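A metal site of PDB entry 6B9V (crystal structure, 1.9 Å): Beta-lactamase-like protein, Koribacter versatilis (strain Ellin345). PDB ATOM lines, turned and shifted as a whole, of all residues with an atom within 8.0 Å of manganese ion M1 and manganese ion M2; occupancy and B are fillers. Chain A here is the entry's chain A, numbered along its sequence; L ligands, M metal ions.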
ATOM      1  N   GLY A  13     -31.357  -7.236 -29.595  1.00  0.00           N
ATOM      2  CA  GLY A  13     -29.975  -7.224 -30.032  1.00  0.00           C
ATOM      3  C   GLY A  13     -28.960  -7.701 -28.985  1.00  0.00           C
ATOM      4  O   GLY A  13     -29.292  -7.942 -27.835  1.00  0.00           O
ATOM      5  N   THR A  14     -27.716  -7.830 -29.417  1.00  0.00           N
ATOM      6  CA  THR A  14     -26.622  -8.233 -28.547  1.00  0.00           C
ATOM      7  C   THR A  14     -26.107  -7.033 -27.702  1.00  0.00           C
ATOM      8  O   THR A  14     -26.706  -5.944 -27.722  1.00  0.00           O
ATOM      9  CB  THR A  14     -25.450  -8.848 -29.372  1.00  0.00           C
ATOM     10  OG1 THR A  14     -24.490  -9.422 -28.469  1.00  0.00           O
ATOM     11  CG2 THR A  14     -24.775  -7.797 -30.266  1.00  0.00           C
ATOM     12  N   SER A  15     -25.003  -7.243 -26.980  1.00  0.00           N
ATOM     13  CA  SER A  15     -24.575  -6.270 -25.954  1.00  0.00           C
ATOM     14  C   SER A  15     -24.193  -4.914 -26.544  1.00  0.00           C
ATOM     15  O   SER A  15     -24.402  -3.883 -25.899  1.00  0.00           O
ATOM     16  CB  SER A  15     -23.395  -6.837 -25.161  1.00  0.00           C
ATOM     17  OG  SER A  15     -22.278  -7.024 -26.000  1.00  0.00           O
ATOM     18  N   MET A  16     -23.643  -4.887 -27.733  1.00  0.00           N
ATOM     19  CA  MET A  16     -23.332  -3.629 -28.392  1.00  0.00           C
ATOM     20  C   MET A  16     -24.423  -3.186 -29.404  1.00  0.00           C
ATOM     21  O   MET A  16     -24.279  -2.201 -30.073  1.00  0.00           O
ATOM     22  CB  MET A  16     -21.967  -3.715 -29.059  1.00  0.00           C
ATOM     23  CG  MET A  16     -20.784  -3.639 -28.111  1.00  0.00           C
ATOM     24  SD  MET A  16     -20.644  -2.173 -26.949  1.00  0.00           S
ATOM     25  CE  MET A  16     -20.979  -0.606 -27.870  1.00  0.00           C
ATOM     26  N   ARG A  39     -30.580  -3.099 -27.016  1.00  0.00           N
ATOM     27  CA  ARG A  39     -30.110  -4.130 -26.122  1.00  0.00           C
ATOM     28  C   ARG A  39     -31.274  -4.999 -25.553  1.00  0.00           C
ATOM     29  O   ARG A  39     -32.380  -4.562 -25.566  1.00  0.00           O
ATOM     30  CB  ARG A  39     -29.206  -3.565 -25.020  1.00  0.00           C
ATOM     31  CG  ARG A  39     -27.716  -3.475 -25.387  1.00  0.00           C
ATOM     32  CD  ARG A  39     -27.432  -2.685 -26.629  1.00  0.00           C
ATOM     33  NE  ARG A  39     -27.481  -1.256 -26.427  1.00  0.00           N
ATOM     34  CZ  ARG A  39     -26.491  -0.506 -26.032  1.00  0.00           C
ATOM     35  NH1 ARG A  39     -25.294  -1.012 -25.781  1.00  0.00           N
ATOM     36  NH2 ARG A  39     -26.671   0.756 -25.843  1.00  0.00           N
ATOM     37  N   PRO A  40     -30.962  -6.205 -25.066  1.00  0.00           N
ATOM     38  CA  PRO A  40     -32.028  -7.207 -24.939  1.00  0.00           C
ATOM     39  C   PRO A  40     -32.908  -7.147 -23.684  1.00  0.00           C
ATOM     40  O   PRO A  40     -32.410  -7.162 -22.561  1.00  0.00           O
ATOM     41  CB  PRO A  40     -31.242  -8.546 -24.992  1.00  0.00           C
ATOM     42  CG  PRO A  40     -29.906  -8.224 -24.392  1.00  0.00           C
ATOM     43  CD  PRO A  40     -29.612  -6.776 -24.834  1.00  0.00           C
ATOM     44  N   ASP A  54     -35.174  -7.172 -17.180  1.00  0.00           N
ATOM     45  CA  ASP A  54     -33.871  -6.496 -17.394  1.00  0.00           C
ATOM     46  C   ASP A  54     -34.033  -5.007 -17.725  1.00  0.00           C
ATOM     47  O   ASP A  54     -35.012  -4.582 -18.323  1.00  0.00           O
ATOM     48  CB  ASP A  54     -33.049  -7.211 -18.485  1.00  0.00           C
ATOM     49  CG  ASP A  54     -32.488  -8.559 -18.008  1.00  0.00           C
ATOM     50  OD1 ASP A  54     -32.439  -8.781 -16.777  1.00  0.00           O
ATOM     51  OD2 ASP A  54     -32.086  -9.382 -18.846  1.00  0.00           O
ATOM     52  N   THR A  77     -32.348 -11.221 -15.267  1.00  0.00           N
ATOM     53  CA  THR A  77     -31.719 -12.487 -15.649  1.00  0.00           C
ATOM     54  C   THR A  77     -30.304 -12.623 -15.051  1.00  0.00           C
ATOM     55  O   THR A  77     -29.930 -13.685 -14.541  1.00  0.00           O
ATOM     56  CB  THR A  77     -31.632 -12.645 -17.194  1.00  0.00           C
ATOM     57  OG1 THR A  77     -30.865 -11.555 -17.734  1.00  0.00           O
ATOM     58  CG2 THR A  77     -33.023 -12.659 -17.825  1.00  0.00           C
ATOM     59  N   HIS A  78     -29.519 -11.534 -15.114  1.00  0.00           N
ATOM     60  CA  HIS A  78     -28.149 -11.524 -14.597  1.00  0.00           C
ATOM     61  C   HIS A  78     -27.604 -10.103 -14.628  1.00  0.00           C
ATOM     62  O   HIS A  78     -28.299  -9.171 -15.028  1.00  0.00           O
ATOM     63  CB  HIS A  78     -27.213 -12.469 -15.383  1.00  0.00           C
ATOM     64  CG  HIS A  78     -26.959 -12.083 -16.811  1.00  0.00           C
ATOM     65  ND1 HIS A  78     -27.989 -11.836 -17.713  1.00  0.00           N
ATOM     66  CD2 HIS A  78     -25.813 -11.957 -17.531  1.00  0.00           C
ATOM     67  CE1 HIS A  78     -27.478 -11.565 -18.893  1.00  0.00           C
ATOM     68  NE2 HIS A  78     -26.163 -11.630 -18.810  1.00  0.00           N
ATOM     69  N   GLY A  79     -26.347  -9.954 -14.215  1.00  0.00           N
ATOM     70  CA  GLY A  79     -25.789  -8.633 -13.917  1.00  0.00           C
ATOM     71  C   GLY A  79     -24.858  -7.974 -14.916  1.00  0.00           C
ATOM     72  O   GLY A  79     -24.250  -6.945 -14.606  1.00  0.00           O
ATOM     73  N   HIS A  80     -24.758  -8.544 -16.119  1.00  0.00           N
ATOM     74  CA  HIS A  80     -23.950  -7.929 -17.175  1.00  0.00           C
ATOM     75  C   HIS A  80     -24.485  -6.550 -17.548  1.00  0.00           C
ATOM     76  O   HIS A  80     -25.665  -6.263 -17.420  1.00  0.00           O
ATOM     77  CB  HIS A  80     -23.892  -8.851 -18.406  1.00  0.00           C
ATOM     78  CG  HIS A  80     -22.956 -10.010 -18.239  1.00  0.00           C
ATOM     79  ND1 HIS A  80     -22.981 -11.117 -19.047  1.00  0.00           N
ATOM     80  CD2 HIS A  80     -21.958 -10.209 -17.348  1.00  0.00           C
ATOM     81  CE1 HIS A  80     -22.047 -11.971 -18.645  1.00  0.00           C
ATOM     82  NE2 HIS A  80     -21.409 -11.446 -17.618  1.00  0.00           N
ATOM     83  N   ALA A  81     -23.577  -5.691 -18.010  1.00  0.00           N
ATOM     84  CA  ALA A  81     -23.894  -4.291 -18.276  1.00  0.00           C
ATOM     85  C   ALA A  81     -25.066  -4.073 -19.234  1.00  0.00           C
ATOM     86  O   ALA A  81     -25.891  -3.156 -19.005  1.00  0.00           O
ATOM     87  CB  ALA A  81     -22.650  -3.588 -18.795  1.00  0.00           C
ATOM     88  N   ASP A  82     -25.156  -4.896 -20.274  1.00  0.00           N
ATOM     89  CA  ASP A  82     -26.216  -4.738 -21.252  1.00  0.00           C
ATOM     90  C   ASP A  82     -27.601  -5.103 -20.694  1.00  0.00           C
ATOM     91  O   ASP A  82     -28.605  -4.888 -21.376  1.00  0.00           O
ATOM     92  CB  ASP A  82     -25.934  -5.542 -22.546  1.00  0.00           C
ATOM     93  CG  ASP A  82     -25.550  -7.009 -22.301  1.00  0.00           C
ATOM     94  OD1 ASP A  82     -24.746  -7.308 -21.395  1.00  0.00           O
ATOM     95  OD2 ASP A  82     -26.044  -7.864 -23.063  1.00  0.00           O
ATOM     96  N   HIS A  83     -27.641  -5.586 -19.443  1.00  0.00           N
ATOM     97  CA  HIS A  83     -28.891  -5.970 -18.797  1.00  0.00           C
ATOM     98  C   HIS A  83     -29.229  -5.120 -17.571  1.00  0.00           C
ATOM     99  O   HIS A  83     -30.327  -5.230 -17.032  1.00  0.00           O
ATOM    100  CB  HIS A  83     -28.820  -7.465 -18.399  1.00  0.00           C
ATOM    101  CG  HIS A  83     -28.587  -8.368 -19.569  1.00  0.00           C
ATOM    102  ND1 HIS A  83     -29.611  -9.046 -20.207  1.00  0.00           N
ATOM    103  CD2 HIS A  83     -27.462  -8.644 -20.277  1.00  0.00           C
ATOM    104  CE1 HIS A  83     -29.124  -9.709 -21.235  1.00  0.00           C
ATOM    105  NE2 HIS A  83     -27.817  -9.499 -21.290  1.00  0.00           N
ATOM    106  N   HIS A 160     -24.283 -19.625 -18.574  1.00  0.00           N
ATOM    107  CA  HIS A 160     -23.801 -18.493 -19.348  1.00  0.00           C
ATOM    108  C   HIS A 160     -22.283 -18.609 -19.261  1.00  0.00           C
ATOM    109  O   HIS A 160     -21.658 -18.032 -18.367  1.00  0.00           O
ATOM    110  CB  HIS A 160     -24.349 -17.174 -18.762  1.00  0.00           C
ATOM    111  CG  HIS A 160     -24.066 -15.933 -19.567  1.00  0.00           C
ATOM    112  ND1 HIS A 160     -23.716 -15.963 -20.900  1.00  0.00           N
ATOM    113  CD2 HIS A 160     -24.168 -14.625 -19.220  1.00  0.00           C
ATOM    114  CE1 HIS A 160     -23.583 -14.708 -21.345  1.00  0.00           C
ATOM    115  NE2 HIS A 160     -23.843 -13.890 -20.354  1.00  0.00           N
ATOM    116  N   ILE A 165     -27.091 -18.463 -14.486  1.00  0.00           N
ATOM    117  CA  ILE A 165     -27.988 -17.297 -14.435  1.00  0.00           C
ATOM    118  C   ILE A 165     -29.423 -17.813 -14.606  1.00  0.00           C
ATOM    119  O   ILE A 165     -29.641 -19.024 -14.677  1.00  0.00           O
ATOM    120  CB  ILE A 165     -27.661 -16.242 -15.536  1.00  0.00           C
ATOM    121  CG1 ILE A 165     -27.982 -16.776 -16.928  1.00  0.00           C
ATOM    122  CG2 ILE A 165     -26.191 -15.821 -15.441  1.00  0.00           C
ATOM    123  CD1 ILE A 165     -28.094 -15.665 -18.003  1.00  0.00           C
ATOM    124  N   THR A 177     -32.273 -15.876 -22.165  1.00  0.00           N
ATOM    125  CA  THR A 177     -31.238 -15.194 -22.943  1.00  0.00           C
ATOM    126  C   THR A 177     -29.874 -15.454 -22.313  1.00  0.00           C
ATOM    127  O   THR A 177     -29.801 -15.947 -21.189  1.00  0.00           O
ATOM    128  CB  THR A 177     -31.510 -13.670 -23.021  1.00  0.00           C
ATOM    129  OG1 THR A 177     -30.526 -13.062 -23.874  1.00  0.00           O
ATOM    130  CG2 THR A 177     -31.474 -13.028 -21.629  1.00  0.00           C
ATOM    131  N   ASP A 178     -28.802 -15.155 -23.061  1.00  0.00           N
ATOM    132  CA  ASP A 178     -27.439 -15.253 -22.533  1.00  0.00           C
ATOM    133  C   ASP A 178     -27.115 -16.633 -21.963  1.00  0.00           C
ATOM    134  O   ASP A 178     -26.749 -16.767 -20.790  1.00  0.00           O
ATOM    135  CB  ASP A 178     -27.185 -14.192 -21.451  1.00  0.00           C
ATOM    136  CG  ASP A 178     -27.180 -12.757 -22.010  1.00  0.00           C
ATOM    137  OD1 ASP A 178     -26.122 -12.106 -22.025  1.00  0.00           O
ATOM    138  OD2 ASP A 178     -28.248 -12.306 -22.435  1.00  0.00           O
ATOM    139  N   PHE A 179     -27.277 -17.672 -22.772  1.00  0.00           N
ATOM    140  CA  PHE A 179     -26.827 -18.977 -22.324  1.00  0.00           C
ATOM    141  C   PHE A 179     -25.978 -19.619 -23.396  1.00  0.00           C
ATOM    142  O   PHE A 179     -26.179 -19.361 -24.590  1.00  0.00           O
ATOM    143  CB  PHE A 179     -27.995 -19.918 -21.978  1.00  0.00           C
ATOM    144  CG  PHE A 179     -28.845 -20.295 -23.159  1.00  0.00           C
ATOM    145  CD1 PHE A 179     -28.493 -21.377 -23.974  1.00  0.00           C
ATOM    146  CD2 PHE A 179     -30.006 -19.586 -23.456  1.00  0.00           C
ATOM    147  CE1 PHE A 179     -29.269 -21.717 -25.074  1.00  0.00           C
ATOM    148  CE2 PHE A 179     -30.798 -19.936 -24.550  1.00  0.00           C
ATOM    149  CZ  PHE A 179     -30.418 -20.990 -25.375  1.00  0.00           C
ATOM    150  N   ASP A 199     -31.611 -17.389 -26.742  1.00  0.00           N
ATOM    151  CA  ASP A 199     -30.374 -16.750 -27.220  1.00  0.00           C
ATOM    152  C   ASP A 199     -29.954 -17.310 -28.584  1.00  0.00           C
ATOM    153  O   ASP A 199     -29.903 -18.530 -28.758  1.00  0.00           O
ATOM    154  CB  ASP A 199     -29.288 -16.997 -26.155  1.00  0.00           C
ATOM    155  CG  ASP A 199     -27.951 -16.357 -26.482  1.00  0.00           C
ATOM    156  OD1 ASP A 199     -27.249 -16.819 -27.398  1.00  0.00           O
ATOM    157  OD2 ASP A 199     -27.587 -15.386 -25.785  1.00  0.00           O
ATOM    158  N   LEU A 201     -26.799 -15.770 -30.911  1.00  0.00           N
ATOM    159  CA  LEU A 201     -25.909 -14.638 -31.100  1.00  0.00           C
ATOM    160  C   LEU A 201     -25.434 -14.497 -32.540  1.00  0.00           C
ATOM    161  O   LEU A 201     -25.420 -13.391 -33.093  1.00  0.00           O
ATOM    162  CB  LEU A 201     -24.700 -14.758 -30.181  1.00  0.00           C
ATOM    163  CG  LEU A 201     -23.601 -13.700 -30.329  1.00  0.00           C
ATOM    164  CD1 LEU A 201     -24.117 -12.348 -29.766  1.00  0.00           C
ATOM    165  CD2 LEU A 201     -22.311 -14.135 -29.619  1.00  0.00           C
ATOM    166  N   THR A 208     -19.906 -17.953 -24.446  1.00  0.00           N
ATOM    167  CA  THR A 208     -20.958 -17.724 -23.454  1.00  0.00           C
ATOM    168  C   THR A 208     -22.351 -17.594 -24.041  1.00  0.00           C
ATOM    169  O   THR A 208     -23.317 -17.378 -23.298  1.00  0.00           O
ATOM    170  CB  THR A 208     -20.668 -16.456 -22.587  1.00  0.00           C
ATOM    171  OG1 THR A 208     -20.618 -15.304 -23.423  1.00  0.00           O
ATOM    172  CG2 THR A 208     -19.337 -16.598 -21.846  1.00  0.00           C
ATOM    173  N   HIS A 209     -22.475 -17.737 -25.365  1.00  0.00           N
ATOM    174  CA  HIS A 209     -23.769 -17.598 -26.024  1.00  0.00           C
ATOM    175  C   HIS A 209     -24.041 -18.841 -26.873  1.00  0.00           C
ATOM    176  O   HIS A 209     -23.212 -19.747 -26.933  1.00  0.00           O
ATOM    177  CB  HIS A 209     -23.834 -16.310 -26.861  1.00  0.00           C
ATOM    178  CG  HIS A 209     -23.907 -15.059 -26.029  1.00  0.00           C
ATOM    179  ND1 HIS A 209     -25.108 -14.520 -25.606  1.00  0.00           N
ATOM    180  CD2 HIS A 209     -22.939 -14.240 -25.534  1.00  0.00           C
ATOM    181  CE1 HIS A 209     -24.884 -13.443 -24.892  1.00  0.00           C
ATOM    182  NE2 HIS A 209     -23.576 -13.238 -24.835  1.00  0.00           N
ATOM    183  N   HIS A 231     -30.979 -11.606 -28.556  1.00  0.00           N
ATOM    184  CA  HIS A 231     -29.561 -11.305 -28.282  1.00  0.00           C
ATOM    185  C   HIS A 231     -28.725 -11.404 -29.576  1.00  0.00           C
ATOM    186  O   HIS A 231     -27.565 -11.792 -29.573  1.00  0.00           O
ATOM    187  CB  HIS A 231     -28.990 -12.231 -27.210  1.00  0.00           C
ATOM    188  CG  HIS A 231     -27.940 -11.593 -26.363  1.00  0.00           C
ATOM    189  ND1 HIS A 231     -26.691 -11.256 -26.846  1.00  0.00           N
ATOM    190  CD2 HIS A 231     -27.952 -11.198 -25.072  1.00  0.00           C
ATOM    191  CE1 HIS A 231     -25.978 -10.698 -25.886  1.00  0.00           C
ATOM    192  NE2 HIS A 231     -26.723 -10.634 -24.801  1.00  0.00           N
HETATM  193  P1  LIG L   1     -23.266 -10.460 -22.594  1.00  0.00           P
HETATM  194  O1  LIG L   1     -24.427 -10.055 -21.680  1.00  0.00           O
HETATM  195  O2  LIG L   1     -23.702 -10.481 -24.025  1.00  0.00           O
HETATM  196  O3  LIG L   1     -22.789 -11.850 -22.227  1.00  0.00           O
HETATM  197  O4  LIG L   1     -22.135  -9.458 -22.449  1.00  0.00           O
HETATM  198 MN    MN M   1     -26.293 -10.045 -22.757  1.00  0.00          MN
HETATM  199 MN    MN M   2     -24.482 -11.736 -20.295  1.00  0.00          MN
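ND1 of His 231 sits close to OG1 of Thr 14, 3.3 Å away.
ND1 of His 83 lies within hydrogen-bond range of OD2 of Asp 54 (2.8 Å).
The side-chain hydroxyl (OG1) of Thr 177 lies within hydrogen-bond range of the side-chain carboxylate (OD2) of Asp 178 (2.8 Å).
The backbone NH of Asp 178 lies within hydrogen-bond range of the side-chain carboxylate of Asp 199.
A ring nitrogen (ND1) of His 78 lies within hydrogen-bond range of the side-chain hydroxyl (OG1) of Thr 77 (2.9 Å).
ND1 of His 160 lies within hydrogen-bond range of O of Thr 208, 2.8 Å away.
The nearest printed residue that does not touch manganese ion M1 is His 209 (4.3 Å).
Of the 24 residues printed, 4 come within 4 Å of manganese ion M2.
The nearest printed residue that does not touch manganese ion M2 is His 83 (4.1 Å).
An oxygen (O1) of the ligand binds manganese ion M1 (2.2 Å).
Manganese ion M1 is bound by NE2 of His 231 (2.2 Å).
Manganese ion M1 is bound by NE2 of His 83 (2.2 Å).
The side-chain carboxylate (OD1) of Asp 178 is bound to manganese ion M1 (2.2 Å).
The side-chain carboxylate (OD2) of Asp 82 binds manganese ion M1, 2.2 Å away.
Manganese ion M1 has five donor atoms within binding distance.
Slightly farther from manganese ion M1 lies O2 of the ligand (2.9 Å).
A ring nitrogen (ND1) of His 80 binds manganese ion M2 (2.0 Å).
O1 of the ligand binds manganese ion M2, at 2.2 Å.
NE2 of His 78 is bound to manganese ion M2.
Manganese ion M2 is bound by a ring nitrogen (NE2) of His 160, 2.2 Å away.
Manganese ion M2 is bound by OD1 of Asp 178, 2.4 Å away.
O3 of the ligand is bound to manganese ion M2.
Manganese ion M2 has six donor atoms within binding distance.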
